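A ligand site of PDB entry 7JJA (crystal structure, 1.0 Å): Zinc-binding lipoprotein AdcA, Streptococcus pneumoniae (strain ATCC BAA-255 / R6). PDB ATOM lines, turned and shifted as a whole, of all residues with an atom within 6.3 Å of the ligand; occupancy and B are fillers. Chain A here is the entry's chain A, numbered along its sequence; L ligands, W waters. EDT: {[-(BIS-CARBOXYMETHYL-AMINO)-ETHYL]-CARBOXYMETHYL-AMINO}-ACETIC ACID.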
ATOM      1  N   ASP A   1      28.200  -0.684   5.773  1.00  0.00           N
ATOM      2  CA  ASP A   1      28.008   0.732   5.470  1.00  0.00           C
ATOM      3  C   ASP A   1      27.715   1.547   6.724  1.00  0.00           C
ATOM      4  O   ASP A   1      26.875   1.176   7.533  1.00  0.00           O
ATOM      5  CB  ASP A   1      26.889   0.919   4.447  1.00  0.00           C
ATOM      6  CG  ASP A   1      27.408   1.068   3.028  1.00  0.00           C
ATOM      7  OD1 ASP A   1      28.644   1.160   2.853  1.00  0.00           O
ATOM      8  OD2 ASP A   1      26.589   1.098   2.093  1.00  0.00           O
ATOM      9  N   GLN A   6      24.067   9.857   3.112  1.00  0.00           N
ATOM     10  CA  GLN A   6      24.283   9.488   1.727  1.00  0.00           C
ATOM     11  C   GLN A   6      24.360   7.979   1.531  1.00  0.00           C
ATOM     12  O   GLN A   6      24.277   7.524   0.387  1.00  0.00           O
ATOM     13  CB  GLN A   6      25.473  10.253   1.137  1.00  0.00           C
ATOM     14  CG  GLN A   6      25.235  11.765   1.162  1.00  0.00           C
ATOM     15  CD  GLN A   6      26.189  12.544   0.291  1.00  0.00           C
ATOM     16  OE1 GLN A   6      27.307  12.096   0.007  1.00  0.00           O
ATOM     17  NE2 GLN A   6      25.766  13.727  -0.114  1.00  0.00           N
ATOM     18  N   ASN A   7      24.447   7.194   2.603  1.00  0.00           N
ATOM     19  CA  ASN A   7      24.249   5.749   2.536  1.00  0.00           C
ATOM     20  C   ASN A   7      22.796   5.348   2.779  1.00  0.00           C
ATOM     21  O   ASN A   7      22.488   4.159   2.777  1.00  0.00           O
ATOM     22  CB  ASN A   7      25.159   5.041   3.543  1.00  0.00           C
ATOM     23  CG  ASN A   7      26.596   4.991   3.084  1.00  0.00           C
ATOM     24  OD1 ASN A   7      26.887   5.145   1.888  1.00  0.00           O
ATOM     25  ND2 ASN A   7      27.509   4.772   4.013  1.00  0.00           N
ATOM     26  N   LYS A  46      35.831  -1.759  -5.821  1.00  0.00           N
ATOM     27  CA  LYS A  46      34.680  -2.066  -4.982  1.00  0.00           C
ATOM     28  C   LYS A  46      34.719  -3.511  -4.502  1.00  0.00           C
ATOM     29  O   LYS A  46      34.455  -3.789  -3.324  1.00  0.00           O
ATOM     30  CB  LYS A  46      33.379  -1.804  -5.743  1.00  0.00           C
ATOM     31  CG  LYS A  46      33.005  -0.336  -5.940  1.00  0.00           C
ATOM     32  CD  LYS A  46      31.625  -0.205  -6.599  1.00  0.00           C
ATOM     33  CE  LYS A  46      31.250   1.225  -6.897  1.00  0.00           C
ATOM     34  NZ  LYS A  46      30.958   2.004  -5.663  1.00  0.00           N
ATOM     35  N   TYR A  61      25.922  -5.761 -12.330  1.00  0.00           N
ATOM     36  CA  TYR A  61      24.972  -4.986 -11.529  1.00  0.00           C
ATOM     37  C   TYR A  61      24.901  -3.539 -12.025  1.00  0.00           C
ATOM     38  O   TYR A  61      23.817  -2.973 -12.177  1.00  0.00           O
ATOM     39  CB  TYR A  61      25.434  -5.068 -10.075  1.00  0.00           C
ATOM     40  CG  TYR A  61      24.708  -4.184  -9.086  1.00  0.00           C
ATOM     41  CD1 TYR A  61      25.284  -3.003  -8.650  1.00  0.00           C
ATOM     42  CD2 TYR A  61      23.492  -4.556  -8.569  1.00  0.00           C
ATOM     43  CE1 TYR A  61      24.641  -2.205  -7.715  1.00  0.00           C
ATOM     44  CE2 TYR A  61      22.836  -3.771  -7.647  1.00  0.00           C
ATOM     45  CZ  TYR A  61      23.419  -2.597  -7.228  1.00  0.00           C
ATOM     46  OH  TYR A  61      22.761  -1.805  -6.311  1.00  0.00           O
ATOM     47  N   TYR A  62      26.064  -2.932 -12.265  1.00  0.00           N
ATOM     48  CA  TYR A  62      26.093  -1.559 -12.766  1.00  0.00           C
ATOM     49  C   TYR A  62      25.743  -1.460 -14.246  1.00  0.00           C
ATOM     50  O   TYR A  62      25.302  -0.397 -14.691  1.00  0.00           O
ATOM     51  CB  TYR A  62      27.448  -0.903 -12.430  1.00  0.00           C
ATOM     52  CG  TYR A  62      27.525  -0.454 -10.990  1.00  0.00           C
ATOM     53  CD1 TYR A  62      26.921   0.730 -10.605  1.00  0.00           C
ATOM     54  CD2 TYR A  62      28.167  -1.192 -10.012  1.00  0.00           C
ATOM     55  CE1 TYR A  62      26.943   1.169  -9.305  1.00  0.00           C
ATOM     56  CE2 TYR A  62      28.192  -0.766  -8.694  1.00  0.00           C
ATOM     57  CZ  TYR A  62      27.576   0.414  -8.348  1.00  0.00           C
ATOM     58  OH  TYR A  62      27.585   0.851  -7.041  1.00  0.00           O
ATOM     59  N   TYR A  66      23.057   1.240 -15.116  1.00  0.00           N
ATOM     60  CA  TYR A  66      23.385   2.421 -15.905  1.00  0.00           C
ATOM     61  C   TYR A  66      22.793   2.426 -17.315  1.00  0.00           C
ATOM     62  O   TYR A  66      22.759   3.481 -17.946  1.00  0.00           O
ATOM     63  CB  TYR A  66      24.905   2.584 -16.015  1.00  0.00           C
ATOM     64  CG  TYR A  66      25.633   2.937 -14.741  1.00  0.00           C
ATOM     65  CD1 TYR A  66      25.029   3.625 -13.707  1.00  0.00           C
ATOM     66  CD2 TYR A  66      26.980   2.618 -14.608  1.00  0.00           C
ATOM     67  CE1 TYR A  66      25.746   3.968 -12.564  1.00  0.00           C
ATOM     68  CE2 TYR A  66      27.701   2.962 -13.487  1.00  0.00           C
ATOM     69  CZ  TYR A  66      27.084   3.632 -12.452  1.00  0.00           C
ATOM     70  OH  TYR A  66      27.819   3.952 -11.338  1.00  0.00           O
ATOM     71  N   TYR A 103      14.600   0.503   0.494  1.00  0.00           N
ATOM     72  CA  TYR A 103      15.202  -0.509  -0.356  1.00  0.00           C
ATOM     73  C   TYR A 103      15.279  -1.836   0.388  1.00  0.00           C
ATOM     74  O   TYR A 103      15.147  -1.909   1.610  1.00  0.00           O
ATOM     75  CB  TYR A 103      16.582  -0.035  -0.817  1.00  0.00           C
ATOM     76  CG  TYR A 103      16.580   1.335  -1.484  1.00  0.00           C
ATOM     77  CD1 TYR A 103      15.816   1.578  -2.615  1.00  0.00           C
ATOM     78  CD2 TYR A 103      17.363   2.368  -0.983  1.00  0.00           C
ATOM     79  CE1 TYR A 103      15.818   2.811  -3.222  1.00  0.00           C
ATOM     80  CE2 TYR A 103      17.373   3.606  -1.588  1.00  0.00           C
ATOM     81  CZ  TYR A 103      16.598   3.823  -2.713  1.00  0.00           C
ATOM     82  OH  TYR A 103      16.609   5.061  -3.319  1.00  0.00           O
ATOM     83  N   ASN A 107      18.169   0.258   3.858  1.00  0.00           N
ATOM     84  CA  ASN A 107      18.401   1.684   3.771  1.00  0.00           C
ATOM     85  C   ASN A 107      17.252   2.332   2.987  1.00  0.00           C
ATOM     86  O   ASN A 107      16.343   1.645   2.504  1.00  0.00           O
ATOM     87  CB  ASN A 107      19.793   1.993   3.197  1.00  0.00           C
ATOM     88  CG  ASN A 107      19.927   1.666   1.709  1.00  0.00           C
ATOM     89  OD1 ASN A 107      19.373   0.671   1.238  1.00  0.00           O
ATOM     90  ND2 ASN A 107      20.667   2.503   0.974  1.00  0.00           N
ATOM     91  N   ARG A 108      17.275   3.659   2.880  1.00  0.00           N
ATOM     92  CA  ARG A 108      16.215   4.409   2.224  1.00  0.00           C
ATOM     93  C   ARG A 108      16.827   5.437   1.278  1.00  0.00           C
ATOM     94  O   ARG A 108      18.035   5.658   1.270  1.00  0.00           O
ATOM     95  CB  ARG A 108      15.340   5.133   3.235  1.00  0.00           C
ATOM     96  CG  ARG A 108      14.677   4.194   4.238  1.00  0.00           C
ATOM     97  CD  ARG A 108      13.586   4.893   5.030  1.00  0.00           C
ATOM     98  NE  ARG A 108      14.105   5.975   5.849  1.00  0.00           N
ATOM     99  CZ  ARG A 108      13.355   6.810   6.552  1.00  0.00           C
ATOM    100  NH1 ARG A 108      12.035   6.703   6.518  1.00  0.00           N
ATOM    101  NH2 ARG A 108      13.921   7.754   7.298  1.00  0.00           N
ATOM    102  N   ARG A 111      13.228  10.332  -3.657  1.00  0.00           N
ATOM    103  CA  ARG A 111      12.980  10.774  -5.035  1.00  0.00           C
ATOM    104  C   ARG A 111      12.384  12.171  -4.996  1.00  0.00           C
ATOM    105  O   ARG A 111      11.416  12.397  -4.264  1.00  0.00           O
ATOM    106  CB  ARG A 111      11.905   9.876  -5.705  1.00  0.00           C
ATOM    107  CG  ARG A 111      12.199   8.379  -5.864  1.00  0.00           C
ATOM    108  CD  ARG A 111      13.222   8.104  -6.975  1.00  0.00           C
ATOM    109  NE  ARG A 111      13.584   6.697  -7.035  1.00  0.00           N
ATOM    110  CZ  ARG A 111      12.919   5.755  -7.709  1.00  0.00           C
ATOM    111  NH1 ARG A 111      11.851   6.068  -8.443  1.00  0.00           N
ATOM    112  NH2 ARG A 111      13.334   4.501  -7.656  1.00  0.00           N
ATOM    113  N   SER A 130      17.226  11.081  -8.009  1.00  0.00           N
ATOM    114  CA  SER A 130      17.781  10.524  -6.782  1.00  0.00           C
ATOM    115  C   SER A 130      19.290  10.770  -6.790  1.00  0.00           C
ATOM    116  O   SER A 130      19.973  10.345  -7.734  1.00  0.00           O
ATOM    117  CB  SER A 130      17.488   9.026  -6.811  1.00  0.00           C
ATOM    118  OG  SER A 130      17.886   8.354  -5.643  1.00  0.00           O
ATOM    119  N   ASP A 131      19.807  11.434  -5.759  1.00  0.00           N
ATOM    120  CA  ASP A 131      21.231  11.795  -5.726  1.00  0.00           C
ATOM    121  C   ASP A 131      21.851  11.527  -4.356  1.00  0.00           C
ATOM    122  O   ASP A 131      22.910  12.078  -4.054  1.00  0.00           O
ATOM    123  CB  ASP A 131      21.500  13.259  -6.119  1.00  0.00           C
ATOM    124  CG  ASP A 131      21.114  14.250  -5.043  1.00  0.00           C
ATOM    125  OD1 ASP A 131      20.154  13.952  -4.297  1.00  0.00           O
ATOM    126  OD2 ASP A 131      21.752  15.337  -4.962  1.00  0.00           O
ATOM    127  N   HIS A 132      21.224  10.685  -3.544  1.00  0.00           N
ATOM    128  CA  HIS A 132      21.673  10.350  -2.188  1.00  0.00           C
ATOM    129  C   HIS A 132      21.635  11.545  -1.238  1.00  0.00           C
ATOM    130  O   HIS A 132      22.185  11.469  -0.136  1.00  0.00           O
ATOM    131  CB  HIS A 132      23.019   9.620  -2.175  1.00  0.00           C
ATOM    132  CG  HIS A 132      22.961   8.264  -2.818  1.00  0.00           C
ATOM    133  ND1 HIS A 132      24.019   7.379  -2.801  1.00  0.00           N
ATOM    134  CD2 HIS A 132      21.949   7.625  -3.475  1.00  0.00           C
ATOM    135  CE1 HIS A 132      23.679   6.274  -3.433  1.00  0.00           C
ATOM    136  NE2 HIS A 132      22.426   6.394  -3.852  1.00  0.00           N
ATOM    137  N   HIS A 143      20.863  10.012 -10.382  1.00  0.00           N
ATOM    138  CA  HIS A 143      20.062   9.048 -11.123  1.00  0.00           C
ATOM    139  C   HIS A 143      18.757   9.716 -11.527  1.00  0.00           C
ATOM    140  O   HIS A 143      18.200  10.515 -10.767  1.00  0.00           O
ATOM    141  CB  HIS A 143      19.678   7.864 -10.240  1.00  0.00           C
ATOM    142  CG  HIS A 143      20.807   7.212  -9.511  1.00  0.00           C
ATOM    143  ND1 HIS A 143      21.946   6.760 -10.138  1.00  0.00           N
ATOM    144  CD2 HIS A 143      20.906   6.841  -8.220  1.00  0.00           C
ATOM    145  CE1 HIS A 143      22.733   6.175  -9.252  1.00  0.00           C
ATOM    146  NE2 HIS A 143      22.124   6.209  -8.083  1.00  0.00           N
ATOM    147  N   PHE A 145      14.760   8.989 -13.351  1.00  0.00           N
ATOM    148  CA  PHE A 145      13.672   8.071 -13.664  1.00  0.00           C
ATOM    149  C   PHE A 145      12.631   8.874 -14.429  1.00  0.00           C
ATOM    150  O   PHE A 145      12.360  10.017 -14.073  1.00  0.00           O
ATOM    151  CB  PHE A 145      13.038   7.510 -12.372  1.00  0.00           C
ATOM    152  CG  PHE A 145      14.045   6.921 -11.418  1.00  0.00           C
ATOM    153  CD1 PHE A 145      14.757   7.724 -10.556  1.00  0.00           C
ATOM    154  CD2 PHE A 145      14.316   5.550 -11.418  1.00  0.00           C
ATOM    155  CE1 PHE A 145      15.721   7.175  -9.711  1.00  0.00           C
ATOM    156  CE2 PHE A 145      15.255   5.003 -10.573  1.00  0.00           C
ATOM    157  CZ  PHE A 145      15.960   5.822  -9.721  1.00  0.00           C
ATOM    158  N   MET A 158      13.638  -0.229  -9.363  1.00  0.00           N
ATOM    159  CA  MET A 158      14.718  -0.263  -8.388  1.00  0.00           C
ATOM    160  C   MET A 158      16.058  -0.699  -8.964  1.00  0.00           C
ATOM    161  O   MET A 158      17.072  -0.516  -8.277  1.00  0.00           O
ATOM    162  CB  MET A 158      14.367  -1.228  -7.253  1.00  0.00           C
ATOM    163  CG  MET A 158      13.247  -0.747  -6.370  1.00  0.00           C
ATOM    164  SD  MET A 158      13.791   0.683  -5.428  1.00  0.00           S
ATOM    165  CE  MET A 158      12.293   1.059  -4.521  1.00  0.00           C
ATOM    166  N   TRP A 161      18.794   2.694 -13.031  1.00  0.00           N
ATOM    167  CA  TRP A 161      18.891   4.052 -12.513  1.00  0.00           C
ATOM    168  C   TRP A 161      19.932   4.789 -13.349  1.00  0.00           C
ATOM    169  O   TRP A 161      21.068   5.020 -12.910  1.00  0.00           O
ATOM    170  CB  TRP A 161      19.214   4.072 -11.001  1.00  0.00           C
ATOM    171  CG  TRP A 161      19.658   2.777 -10.410  1.00  0.00           C
ATOM    172  CD1 TRP A 161      18.855   1.856  -9.809  1.00  0.00           C
ATOM    173  CD2 TRP A 161      20.996   2.250 -10.345  1.00  0.00           C
ATOM    174  NE1 TRP A 161      19.595   0.785  -9.377  1.00  0.00           N
ATOM    175  CE2 TRP A 161      20.910   1.001  -9.687  1.00  0.00           C
ATOM    176  CE3 TRP A 161      22.247   2.708 -10.764  1.00  0.00           C
ATOM    177  CZ2 TRP A 161      22.039   0.215  -9.456  1.00  0.00           C
ATOM    178  CZ3 TRP A 161      23.356   1.929 -10.510  1.00  0.00           C
ATOM    179  CH2 TRP A 161      23.259   0.688  -9.872  1.00  0.00           C
ATOM    180  N   THR A 163      22.450   7.225 -14.887  1.00  0.00           N
ATOM    181  CA  THR A 163      23.256   8.067 -14.023  1.00  0.00           C
ATOM    182  C   THR A 163      24.037   9.090 -14.829  1.00  0.00           C
ATOM    183  O   THR A 163      24.592   8.775 -15.891  1.00  0.00           O
ATOM    184  CB  THR A 163      24.184   7.163 -13.184  1.00  0.00           C
ATOM    185  OG1 THR A 163      23.376   6.311 -12.368  1.00  0.00           O
ATOM    186  CG2 THR A 163      25.107   7.945 -12.275  1.00  0.00           C
HETATM  187  O20 EDT L   1      24.682   4.447  -7.708  1.00  0.00           O
HETATM  188  C5  EDT L   1      23.978   3.856  -6.860  1.00  0.00           C
HETATM  189  O19 EDT L   1      22.995   4.399  -6.271  1.00  0.00           O
HETATM  190  C4  EDT L   1      24.280   2.388  -6.555  1.00  0.00           C
HETATM  191  N3  EDT L   1      23.603   1.988  -5.316  1.00  0.00           N
HETATM  192  C2  EDT L   1      24.541   1.236  -4.479  1.00  0.00           C
HETATM  193  C1  EDT L   1      25.581   2.185  -3.882  1.00  0.00           C
HETATM  194  O18 EDT L   1      26.567   1.713  -3.271  1.00  0.00           O
HETATM  195  O17 EDT L   1      25.417   3.436  -4.007  1.00  0.00           O
HETATM  196  C6  EDT L   1      22.411   1.150  -5.570  1.00  0.00           C
HETATM  197  C7  EDT L   1      21.288   1.845  -6.375  1.00  0.00           C
HETATM  198  N8  EDT L   1      20.648   2.971  -5.638  1.00  0.00           N
HETATM  199  C9  EDT L   1      20.051   2.556  -4.355  1.00  0.00           C
HETATM  200  C10 EDT L   1      21.025   2.747  -3.206  1.00  0.00           C
HETATM  201  O16 EDT L   1      22.121   3.341  -3.424  1.00  0.00           O
HETATM  202  O15 EDT L   1      20.719   2.306  -2.061  1.00  0.00           O
HETATM  203  C11 EDT L   1      19.630   3.590  -6.515  1.00  0.00           C
HETATM  204  C12 EDT L   1      19.333   5.015  -6.067  1.00  0.00           C
HETATM  205  O13 EDT L   1      20.126   5.522  -5.254  1.00  0.00           O
HETATM  206  O14 EDT L   1      18.320   5.638  -6.518  1.00  0.00           O
HETATM  207  O   HOH W   1      26.472   5.250  -9.443  1.00  0.00           O
HETATM  208  O   HOH W   2      25.865   4.729  -0.865  1.00  0.00           O
HETATM  209  O   HOH W   3      27.457  -1.014  -5.053  1.00  0.00           O
HETATM  210  O   HOH W   4      23.593   3.057  -1.098  1.00  0.00           O
HETATM  211  O   HOH W   5      19.740  -0.285  -1.847  1.00  0.00           O
HETATM  212  O   HOH W   6      17.277   1.244  -6.132  1.00  0.00           O
HETATM  213  O   HOH W   7      27.139   5.328  -4.299  1.00  0.00           O
HETATM  214  O   HOH W   8      18.901   6.371  -2.957  1.00  0.00           O
HETATM  215  O   HOH W   9      22.328   5.000  -0.373  1.00  0.00           O
HETATM  216  O   HOH W  10      22.410  -0.909  -2.791  1.00  0.00           O
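A ring nitrogen (NE2) of His 143 sits at hydrogen-bond distance from an oxygen (O19) of the ligand. A ring nitrogen (NE2) of His 132 is in hydrogen-bond range of an oxygen (O13) of the ligand, at 2.8 Å. O14 of the ligand is in hydrogen-bond range of OG of Ser 130 (2.9 Å). O15 of the ligand lies within hydrogen-bond range of ND2 of Asn 107 (3.0 Å).
The backbone NH of His 143 lies within hydrogen-bond range of the backbone carbonyl oxygen of Ser 130, at 2.8 Å. A ring nitrogen (ND1) of His 143 lies within hydrogen-bond range of the backbone carbonyl oxygen (O) of Trp 161. OG1 of Thr 163 is in hydrogen-bond range of ND1 of His 143, at 2.7 Å. ND1 of His 132 lies within hydrogen-bond range of O of Gln 6. The side-chain amide nitrogen of Asn 107 sits at hydrogen-bond distance from the backbone carbonyl oxygen of Asn 7, at 3.1 Å. The indole nitrogen of Trp 161 sits at hydrogen-bond distance from the backbone carbonyl oxygen of Met 158 (3.0 Å). The backbone carbonyl oxygen of Trp 161 is in hydrogen-bond range of the side-chain hydroxyl of Thr 163 (2.7 Å).
Residues that only touch the ligand: Tyr 61 (3.1 Å), Trp 161 (3.4 Å), Tyr 103 (3.5 Å), Tyr 62 (3.7 Å) and Phe 145 (3.98 Å). Nine residues have an atom within 4 Å of the ligand: Tyr 61, Tyr 62, Tyr 103, Asn 107, Ser 130, His 132, His 143, Phe 145 and Trp 161.
Water W1 lies within hydrogen-bond range of an oxygen (O20) of the ligand (2.6 Å) and the side-chain hydroxyl (OH) of Tyr 66 (2.7 Å). Water W8 lies within hydrogen-bond range of OH of Tyr 103 (2.7 Å), O13 of the ligand (2.7 Å) and OG of Ser 130 (3.5 Å). Water W5 bridges O15 of the ligand (2.8 Å) and OD1 of Asn 107 (3.3 Å). Water W3 lies within hydrogen-bond range of OH of Tyr 62 (2.7 Å) and O18 of the ligand (3.4 Å). Water W2 lies within hydrogen-bond range of the side-chain amide oxygen of Asn 7, an oxygen (O17) of the ligand and the backbone carbonyl oxygen of Gln 6. Water W9 lies within hydrogen-bond range of the backbone carbonyl oxygen (O) of Asn 7 (3.3 Å), the backbone carbonyl oxygen (O) of Gln 6 (3.3 Å), the side-chain amide nitrogen (ND2) of Asn 107 (3.3 Å) and an oxygen (O16) of the ligand (3.5 Å).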
